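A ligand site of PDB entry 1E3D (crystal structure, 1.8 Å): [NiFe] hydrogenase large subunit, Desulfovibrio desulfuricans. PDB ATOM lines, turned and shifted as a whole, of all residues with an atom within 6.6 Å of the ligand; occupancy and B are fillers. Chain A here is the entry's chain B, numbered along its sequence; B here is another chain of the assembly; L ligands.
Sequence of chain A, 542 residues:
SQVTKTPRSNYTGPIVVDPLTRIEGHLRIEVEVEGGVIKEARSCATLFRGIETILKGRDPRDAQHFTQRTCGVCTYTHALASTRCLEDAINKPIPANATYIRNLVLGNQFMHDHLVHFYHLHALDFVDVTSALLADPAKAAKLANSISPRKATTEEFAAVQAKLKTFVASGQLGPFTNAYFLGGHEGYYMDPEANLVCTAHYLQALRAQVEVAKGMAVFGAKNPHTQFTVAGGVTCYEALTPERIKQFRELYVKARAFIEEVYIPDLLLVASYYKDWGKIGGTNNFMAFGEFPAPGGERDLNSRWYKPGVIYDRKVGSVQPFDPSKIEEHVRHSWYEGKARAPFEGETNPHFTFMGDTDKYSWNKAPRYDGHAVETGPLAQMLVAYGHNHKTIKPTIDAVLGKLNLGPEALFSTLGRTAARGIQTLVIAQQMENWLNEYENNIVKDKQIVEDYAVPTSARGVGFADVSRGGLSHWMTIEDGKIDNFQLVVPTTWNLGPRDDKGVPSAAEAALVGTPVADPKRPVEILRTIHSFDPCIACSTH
The backbone NH of Thr 492 is in hydrogen-bond range of an oxygen (O3) of the ligand, 3.1 Å away. N of Arg 469 is in hydrogen-bond range of O1 of the ligand, 3.1 Å away. FE1 of the ligand is bound by SG of Cys 539, at 2.3 Å. The side-chain hydroxyl (OG1) of Thr 492 sits at hydrogen-bond distance from an oxygen (O3) of the ligand (2.8 Å). NI1 of the ligand is bound by SG of Cys 71. A sulfur (S1) of the ligand sits close to the guanidinium group of Arg 469 (3.1 Å). A ring nitrogen (NE2) of His 78 lies close to an oxygen (O2) of the ligand. NI1 of the ligand is bound by SG of Cys 536. SG of Cys 74 binds FE1 of the ligand (2.3 Å).
The side-chain sulfur of Cys 71 lies close to the backbone NH of Val 73. ND1 of His 78 lies within hydrogen-bond range of NE2 of His 474 (3.0 Å). N of Cys 536 sits at hydrogen-bond distance from OG1 of Thr 492. NH1 of Arg 469 lies within salt-bridge range of OD2 of Asp 113, 2.8 Å away. SG of Cys 536 lies close to OE1 of Glu 24, 3.1 Å away. SG of Cys 539 sits close to NE2 of His 78 (3.3 Å). O of Cys 74 sits at hydrogen-bond distance from OG1 of Thr 77 (2.8 Å). The side-chain carboxylate of Asp 534 lies within salt-bridge range of the guanidinium group of Arg 469.
Thr 77 touches the ligand. Val 467 touches the ligand. Ser 468 touches the ligand. Leu 472 touches the ligand. Val 490 touches the ligand. CD of Pro 491 touches O2 of the ligand, 3.5 Å away. Hydrophobic or aromatic side chains that line the ligand: His 78, Val 467, Leu 472, Val 490 and Pro 491. 13 residues have an atom within 4 Å of the ligand: Cys 71, Cys 74, Thr 77, His 78, Val 467, Ser 468, Arg 469, Leu 472, Val 490, Pro 491, Thr 492, Cys 536 and Cys 539.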
ATOM      1  N   GLU A  24      36.324  23.810   5.851  1.00  0.00           N
ATOM      2  CA  GLU A  24      35.241  23.414   4.967  1.00  0.00           C
ATOM      3  C   GLU A  24      35.386  24.243   3.691  1.00  0.00           C
ATOM      4  O   GLU A  24      35.650  25.441   3.739  1.00  0.00           O
ATOM      5  CB  GLU A  24      33.862  23.621   5.597  1.00  0.00           C
ATOM      6  CG  GLU A  24      32.679  23.092   4.813  1.00  0.00           C
ATOM      7  CD  GLU A  24      32.325  23.760   3.510  1.00  0.00           C
ATOM      8  OE1 GLU A  24      32.541  25.000   3.419  1.00  0.00           O
ATOM      9  OE2 GLU A  24      31.885  23.074   2.561  1.00  0.00           O
ATOM     10  N   THR A  70      23.501  25.417   2.561  1.00  0.00           N
ATOM     11  CA  THR A  70      24.688  26.253   2.530  1.00  0.00           C
ATOM     12  C   THR A  70      25.908  25.552   3.115  1.00  0.00           C
ATOM     13  O   THR A  70      27.041  25.621   2.600  1.00  0.00           O
ATOM     14  CB  THR A  70      24.447  27.572   3.329  1.00  0.00           C
ATOM     15  OG1 THR A  70      23.463  28.382   2.678  1.00  0.00           O
ATOM     16  CG2 THR A  70      25.749  28.338   3.405  1.00  0.00           C
ATOM     17  N   CYS A  71      25.696  24.825   4.219  1.00  0.00           N
ATOM     18  CA  CYS A  71      26.810  24.161   4.908  1.00  0.00           C
ATOM     19  C   CYS A  71      26.383  23.037   5.837  1.00  0.00           C
ATOM     20  O   CYS A  71      25.421  23.181   6.584  1.00  0.00           O
ATOM     21  CB  CYS A  71      27.593  25.172   5.762  1.00  0.00           C
ATOM     22  SG  CYS A  71      29.201  24.524   6.283  1.00  0.00           S
ATOM     23  N   GLY A  72      27.108  21.922   5.825  1.00  0.00           N
ATOM     24  CA  GLY A  72      26.797  20.804   6.670  1.00  0.00           C
ATOM     25  C   GLY A  72      27.743  20.619   7.860  1.00  0.00           C
ATOM     26  O   GLY A  72      27.466  19.765   8.701  1.00  0.00           O
ATOM     27  N   VAL A  73      28.822  21.380   7.931  1.00  0.00           N
ATOM     28  CA  VAL A  73      29.644  21.465   9.140  1.00  0.00           C
ATOM     29  C   VAL A  73      28.864  22.265  10.175  1.00  0.00           C
ATOM     30  O   VAL A  73      28.543  21.742  11.251  1.00  0.00           O
ATOM     31  CB  VAL A  73      31.033  22.044   8.847  1.00  0.00           C
ATOM     32  CG1 VAL A  73      31.823  22.346  10.105  1.00  0.00           C
ATOM     33  CG2 VAL A  73      31.847  21.108   7.957  1.00  0.00           C
ATOM     34  N   CYS A  74      28.525  23.511   9.833  1.00  0.00           N
ATOM     35  CA  CYS A  74      27.618  24.342  10.608  1.00  0.00           C
ATOM     36  C   CYS A  74      26.189  24.022  10.164  1.00  0.00           C
ATOM     37  O   CYS A  74      25.396  24.879   9.802  1.00  0.00           O
ATOM     38  CB  CYS A  74      27.909  25.818  10.483  1.00  0.00           C
ATOM     39  SG  CYS A  74      27.711  26.653   8.908  1.00  0.00           S
ATOM     40  N   THR A  75      25.870  22.732  10.173  1.00  0.00           N
ATOM     41  CA  THR A  75      24.496  22.269   9.971  1.00  0.00           C
ATOM     42  C   THR A  75      23.552  22.892  10.993  1.00  0.00           C
ATOM     43  O   THR A  75      24.013  23.361  12.040  1.00  0.00           O
ATOM     44  CB  THR A  75      24.497  20.733  10.020  1.00  0.00           C
ATOM     45  OG1 THR A  75      23.147  20.302   9.760  1.00  0.00           O
ATOM     46  CG2 THR A  75      24.735  20.151  11.395  1.00  0.00           C
ATOM     47  N   THR A  77      22.392  25.721  11.701  1.00  0.00           N
ATOM     48  CA  THR A  77      22.521  27.149  11.840  1.00  0.00           C
ATOM     49  C   THR A  77      21.706  27.921  10.795  1.00  0.00           C
ATOM     50  O   THR A  77      21.045  28.882  11.187  1.00  0.00           O
ATOM     51  CB  THR A  77      23.995  27.645  11.792  1.00  0.00           C
ATOM     52  OG1 THR A  77      24.566  27.446  10.499  1.00  0.00           O
ATOM     53  CG2 THR A  77      24.863  26.873  12.789  1.00  0.00           C
ATOM     54  N   HIS A  78      21.771  27.542   9.530  1.00  0.00           N
ATOM     55  CA  HIS A  78      21.118  28.300   8.454  1.00  0.00           C
ATOM     56  C   HIS A  78      19.612  28.080   8.487  1.00  0.00           C
ATOM     57  O   HIS A  78      18.864  28.996   8.175  1.00  0.00           O
ATOM     58  CB  HIS A  78      21.728  27.975   7.078  1.00  0.00           C
ATOM     59  CG  HIS A  78      23.111  28.551   6.896  1.00  0.00           C
ATOM     60  ND1 HIS A  78      23.353  29.877   6.631  1.00  0.00           N
ATOM     61  CD2 HIS A  78      24.324  27.967   6.962  1.00  0.00           C
ATOM     62  CE1 HIS A  78      24.652  30.081   6.526  1.00  0.00           C
ATOM     63  NE2 HIS A  78      25.287  28.926   6.732  1.00  0.00           N
ATOM     64  N   ASP A 113      30.661  21.043  16.926  1.00  0.00           N
ATOM     65  CA  ASP A 113      31.477  21.731  15.926  1.00  0.00           C
ATOM     66  C   ASP A 113      32.828  22.126  16.495  1.00  0.00           C
ATOM     67  O   ASP A 113      33.891  21.881  15.903  1.00  0.00           O
ATOM     68  CB  ASP A 113      30.628  22.886  15.437  1.00  0.00           C
ATOM     69  CG  ASP A 113      31.084  23.565  14.172  1.00  0.00           C
ATOM     70  OD1 ASP A 113      32.237  23.346  13.734  1.00  0.00           O
ATOM     71  OD2 ASP A 113      30.256  24.322  13.632  1.00  0.00           O
ATOM     72  N   VAL A 467      26.760  32.109  15.686  1.00  0.00           N
ATOM     73  CA  VAL A 467      26.932  30.653  15.641  1.00  0.00           C
ATOM     74  C   VAL A 467      28.397  30.296  15.755  1.00  0.00           C
ATOM     75  O   VAL A 467      29.200  31.172  16.111  1.00  0.00           O
ATOM     76  CB  VAL A 467      26.260  30.063  14.388  1.00  0.00           C
ATOM     77  CG1 VAL A 467      24.743  30.259  14.461  1.00  0.00           C
ATOM     78  CG2 VAL A 467      26.772  30.662  13.090  1.00  0.00           C
ATOM     79  N   SER A 468      28.820  29.073  15.490  1.00  0.00           N
ATOM     80  CA  SER A 468      30.178  28.609  15.666  1.00  0.00           C
ATOM     81  C   SER A 468      31.235  29.578  15.148  1.00  0.00           C
ATOM     82  O   SER A 468      32.245  29.783  15.834  1.00  0.00           O
ATOM     83  CB  SER A 468      30.415  27.263  14.958  1.00  0.00           C
ATOM     84  OG  SER A 468      29.553  26.268  15.483  1.00  0.00           O
ATOM     85  N   ARG A 469      31.023  30.133  13.973  1.00  0.00           N
ATOM     86  CA  ARG A 469      32.048  31.008  13.398  1.00  0.00           C
ATOM     87  C   ARG A 469      31.766  32.493  13.470  1.00  0.00           C
ATOM     88  O   ARG A 469      32.594  33.303  12.993  1.00  0.00           O
ATOM     89  CB  ARG A 469      32.280  30.567  11.938  1.00  0.00           C
ATOM     90  CG  ARG A 469      33.049  29.251  11.924  1.00  0.00           C
ATOM     91  CD  ARG A 469      32.826  28.471  10.635  1.00  0.00           C
ATOM     92  NE  ARG A 469      33.265  27.104  10.845  1.00  0.00           N
ATOM     93  CZ  ARG A 469      32.598  26.086  11.333  1.00  0.00           C
ATOM     94  NH1 ARG A 469      31.333  26.129  11.710  1.00  0.00           N
ATOM     95  NH2 ARG A 469      33.240  24.924  11.452  1.00  0.00           N
ATOM     96  N   GLY A 470      30.628  32.870  14.041  1.00  0.00           N
ATOM     97  CA  GLY A 470      30.334  34.273  14.247  1.00  0.00           C
ATOM     98  C   GLY A 470      28.963  34.725  13.814  1.00  0.00           C
ATOM     99  O   GLY A 470      28.031  33.936  13.897  1.00  0.00           O
ATOM    100  N   GLY A 471      28.861  35.984  13.408  1.00  0.00           N
ATOM    101  CA  GLY A 471      27.591  36.643  13.128  1.00  0.00           C
ATOM    102  C   GLY A 471      26.998  36.295  11.783  1.00  0.00           C
ATOM    103  O   GLY A 471      27.494  36.711  10.733  1.00  0.00           O
ATOM    104  N   LEU A 472      25.928  35.508  11.807  1.00  0.00           N
ATOM    105  CA  LEU A 472      25.157  35.078  10.667  1.00  0.00           C
ATOM    106  C   LEU A 472      23.846  35.866  10.564  1.00  0.00           C
ATOM    107  O   LEU A 472      23.141  36.067  11.536  1.00  0.00           O
ATOM    108  CB  LEU A 472      24.812  33.597  10.774  1.00  0.00           C
ATOM    109  CG  LEU A 472      23.844  33.028   9.754  1.00  0.00           C
ATOM    110  CD1 LEU A 472      24.360  33.111   8.334  1.00  0.00           C
ATOM    111  CD2 LEU A 472      23.502  31.570  10.118  1.00  0.00           C
ATOM    112  N   HIS A 474      20.359  36.422   7.818  1.00  0.00           N
ATOM    113  CA  HIS A 474      19.577  36.195   6.623  1.00  0.00           C
ATOM    114  C   HIS A 474      18.522  37.311   6.455  1.00  0.00           C
ATOM    115  O   HIS A 474      17.788  37.645   7.383  1.00  0.00           O
ATOM    116  CB  HIS A 474      18.856  34.853   6.647  1.00  0.00           C
ATOM    117  CG  HIS A 474      19.703  33.630   6.614  1.00  0.00           C
ATOM    118  ND1 HIS A 474      19.112  32.403   6.454  1.00  0.00           N
ATOM    119  CD2 HIS A 474      21.026  33.377   6.718  1.00  0.00           C
ATOM    120  CE1 HIS A 474      20.029  31.442   6.445  1.00  0.00           C
ATOM    121  NE2 HIS A 474      21.210  32.016   6.610  1.00  0.00           N
ATOM    122  N   VAL A 489      24.449  36.814   4.744  1.00  0.00           N
ATOM    123  CA  VAL A 489      25.731  37.409   5.138  1.00  0.00           C
ATOM    124  C   VAL A 489      26.253  36.524   6.269  1.00  0.00           C
ATOM    125  O   VAL A 489      25.634  36.444   7.339  1.00  0.00           O
ATOM    126  CB  VAL A 489      25.618  38.893   5.517  1.00  0.00           C
ATOM    127  CG1 VAL A 489      26.999  39.539   5.618  1.00  0.00           C
ATOM    128  CG2 VAL A 489      24.755  39.641   4.514  1.00  0.00           C
ATOM    129  N   VAL A 490      27.337  35.821   6.011  1.00  0.00           N
ATOM    130  CA  VAL A 490      27.724  34.641   6.800  1.00  0.00           C
ATOM    131  C   VAL A 490      29.057  34.905   7.487  1.00  0.00           C
ATOM    132  O   VAL A 490      29.841  35.702   6.962  1.00  0.00           O
ATOM    133  CB  VAL A 490      27.710  33.435   5.853  1.00  0.00           C
ATOM    134  CG1 VAL A 490      27.895  32.091   6.534  1.00  0.00           C
ATOM    135  CG2 VAL A 490      26.390  33.378   5.063  1.00  0.00           C
ATOM    136  N   PRO A 491      29.316  34.360   8.673  1.00  0.00           N
ATOM    137  CA  PRO A 491      30.526  34.675   9.445  1.00  0.00           C
ATOM    138  C   PRO A 491      31.821  34.619   8.634  1.00  0.00           C
ATOM    139  O   PRO A 491      32.610  35.566   8.688  1.00  0.00           O
ATOM    140  CB  PRO A 491      30.531  33.622  10.560  1.00  0.00           C
ATOM    141  CG  PRO A 491      29.082  33.336  10.784  1.00  0.00           C
ATOM    142  CD  PRO A 491      28.428  33.448   9.434  1.00  0.00           C
ATOM    143  N   THR A 492      32.053  33.544   7.900  1.00  0.00           N
ATOM    144  CA  THR A 492      33.302  33.423   7.113  1.00  0.00           C
ATOM    145  C   THR A 492      33.304  34.403   5.952  1.00  0.00           C
ATOM    146  O   THR A 492      34.379  34.803   5.489  1.00  0.00           O
ATOM    147  CB  THR A 492      33.496  31.984   6.633  1.00  0.00           C
ATOM    148  OG1 THR A 492      33.549  31.079   7.738  1.00  0.00           O
ATOM    149  CG2 THR A 492      34.846  31.866   5.927  1.00  0.00           C
ATOM    150  N   THR A 493      32.149  34.867   5.473  1.00  0.00           N
ATOM    151  CA  THR A 493      32.135  36.026   4.581  1.00  0.00           C
ATOM    152  C   THR A 493      32.885  37.227   5.175  1.00  0.00           C
ATOM    153  O   THR A 493      33.677  37.894   4.488  1.00  0.00           O
ATOM    154  CB  THR A 493      30.716  36.506   4.242  1.00  0.00           C
ATOM    155  OG1 THR A 493      29.853  35.413   3.979  1.00  0.00           O
ATOM    156  CG2 THR A 493      30.814  37.344   2.967  1.00  0.00           C
ATOM    157  N   ASP A 534      38.618  29.275  11.690  1.00  0.00           N
ATOM    158  CA  ASP A 534      37.672  28.201  11.377  1.00  0.00           C
ATOM    159  C   ASP A 534      36.796  28.534  10.158  1.00  0.00           C
ATOM    160  O   ASP A 534      35.576  28.631  10.245  1.00  0.00           O
ATOM    161  CB  ASP A 534      36.831  27.950  12.612  1.00  0.00           C
ATOM    162  CG  ASP A 534      35.881  26.782  12.570  1.00  0.00           C
ATOM    163  OD1 ASP A 534      36.015  25.939  11.650  1.00  0.00           O
ATOM    164  OD2 ASP A 534      35.024  26.729  13.491  1.00  0.00           O
ATOM    165  N   PRO A 535      37.440  28.721   9.020  1.00  0.00           N
ATOM    166  CA  PRO A 535      36.740  29.133   7.808  1.00  0.00           C
ATOM    167  C   PRO A 535      35.925  28.000   7.185  1.00  0.00           C
ATOM    168  O   PRO A 535      36.330  26.850   7.111  1.00  0.00           O
ATOM    169  CB  PRO A 535      37.864  29.468   6.826  1.00  0.00           C
ATOM    170  CG  PRO A 535      39.149  29.090   7.451  1.00  0.00           C
ATOM    171  CD  PRO A 535      38.880  28.519   8.798  1.00  0.00           C
ATOM    172  N   CYS A 536      34.760  28.436   6.725  1.00  0.00           N
ATOM    173  CA  CYS A 536      33.881  27.609   5.923  1.00  0.00           C
ATOM    174  C   CYS A 536      33.516  28.390   4.670  1.00  0.00           C
ATOM    175  O   CYS A 536      32.843  29.426   4.730  1.00  0.00           O
ATOM    176  CB  CYS A 536      32.668  27.307   6.826  1.00  0.00           C
ATOM    177  SG  CYS A 536      31.448  26.299   5.982  1.00  0.00           S
ATOM    178  N   ILE A 537      34.005  27.881   3.542  1.00  0.00           N
ATOM    179  CA  ILE A 537      33.837  28.622   2.267  1.00  0.00           C
ATOM    180  C   ILE A 537      32.523  28.319   1.580  1.00  0.00           C
ATOM    181  O   ILE A 537      32.022  29.118   0.781  1.00  0.00           O
ATOM    182  CB  ILE A 537      35.081  28.331   1.389  1.00  0.00           C
ATOM    183  CG1 ILE A 537      36.371  28.509   2.188  1.00  0.00           C
ATOM    184  CG2 ILE A 537      35.086  29.174   0.127  1.00  0.00           C
ATOM    185  CD1 ILE A 537      36.582  29.904   2.749  1.00  0.00           C
ATOM    186  N   ALA A 538      31.875  27.174   1.866  1.00  0.00           N
ATOM    187  CA  ALA A 538      30.516  26.920   1.394  1.00  0.00           C
ATOM    188  C   ALA A 538      29.581  27.967   2.000  1.00  0.00           C
ATOM    189  O   ALA A 538      28.712  28.561   1.362  1.00  0.00           O
ATOM    190  CB  ALA A 538      30.053  25.529   1.762  1.00  0.00           C
ATOM    191  N   CYS A 539      29.805  28.185   3.302  1.00  0.00           N
ATOM    192  CA  CYS A 539      29.170  29.244   4.063  1.00  0.00           C
ATOM    193  C   CYS A 539      29.412  30.643   3.500  1.00  0.00           C
ATOM    194  O   CYS A 539      28.465  31.389   3.211  1.00  0.00           O
ATOM    195  CB  CYS A 539      29.656  29.217   5.534  1.00  0.00           C
ATOM    196  SG  CYS A 539      28.528  28.346   6.630  1.00  0.00           S
ATOM    197  N   SER A 540      30.679  31.015   3.348  1.00  0.00           N
ATOM    198  CA  SER A 540      31.069  32.382   3.026  1.00  0.00           C
ATOM    199  C   SER A 540      30.585  32.812   1.652  1.00  0.00           C
ATOM    200  O   SER A 540      30.142  33.961   1.545  1.00  0.00           O
ATOM    201  CB  SER A 540      32.581  32.588   3.160  1.00  0.00           C
ATOM    202  OG  SER A 540      33.340  31.913   2.175  1.00  0.00           O
ATOM    203  N   CYS B  17      28.311  20.959   0.238  1.00  0.00           N
ATOM    204  CA  CYS B  17      28.190  21.665   1.503  1.00  0.00           C
ATOM    205  C   CYS B  17      28.914  20.951   2.625  1.00  0.00           C
ATOM    206  O   CYS B  17      28.935  21.407   3.763  1.00  0.00           O
ATOM    207  CB  CYS B  17      26.716  21.968   1.845  1.00  0.00           C
ATOM    208  SG  CYS B  17      25.870  20.746   2.877  1.00  0.00           S
HETATM  209 NI1  LIG L   1      29.770  26.281   7.415  1.00  0.00          NI
HETATM  210 FE1  LIG L   1      28.852  28.623   8.864  1.00  0.00          FE
HETATM  211  C1  LIG L   1      29.077  28.627  10.710  1.00  0.00           C
HETATM  212  C2  LIG L   1      27.392  29.674   9.039  1.00  0.00           C
HETATM  213  C3  LIG L   1      30.020  29.958   8.575  1.00  0.00           C
HETATM  214  O1  LIG L   1      29.320  28.792  11.790  1.00  0.00           O
HETATM  215  O2  LIG L   1      26.703  30.454   9.368  1.00  0.00           O
HETATM  216  O3  LIG L   1      30.803  30.787   8.409  1.00  0.00           O
HETATM  217  S1  LIG L   1      30.614  27.186   8.869  1.00  0.00           S
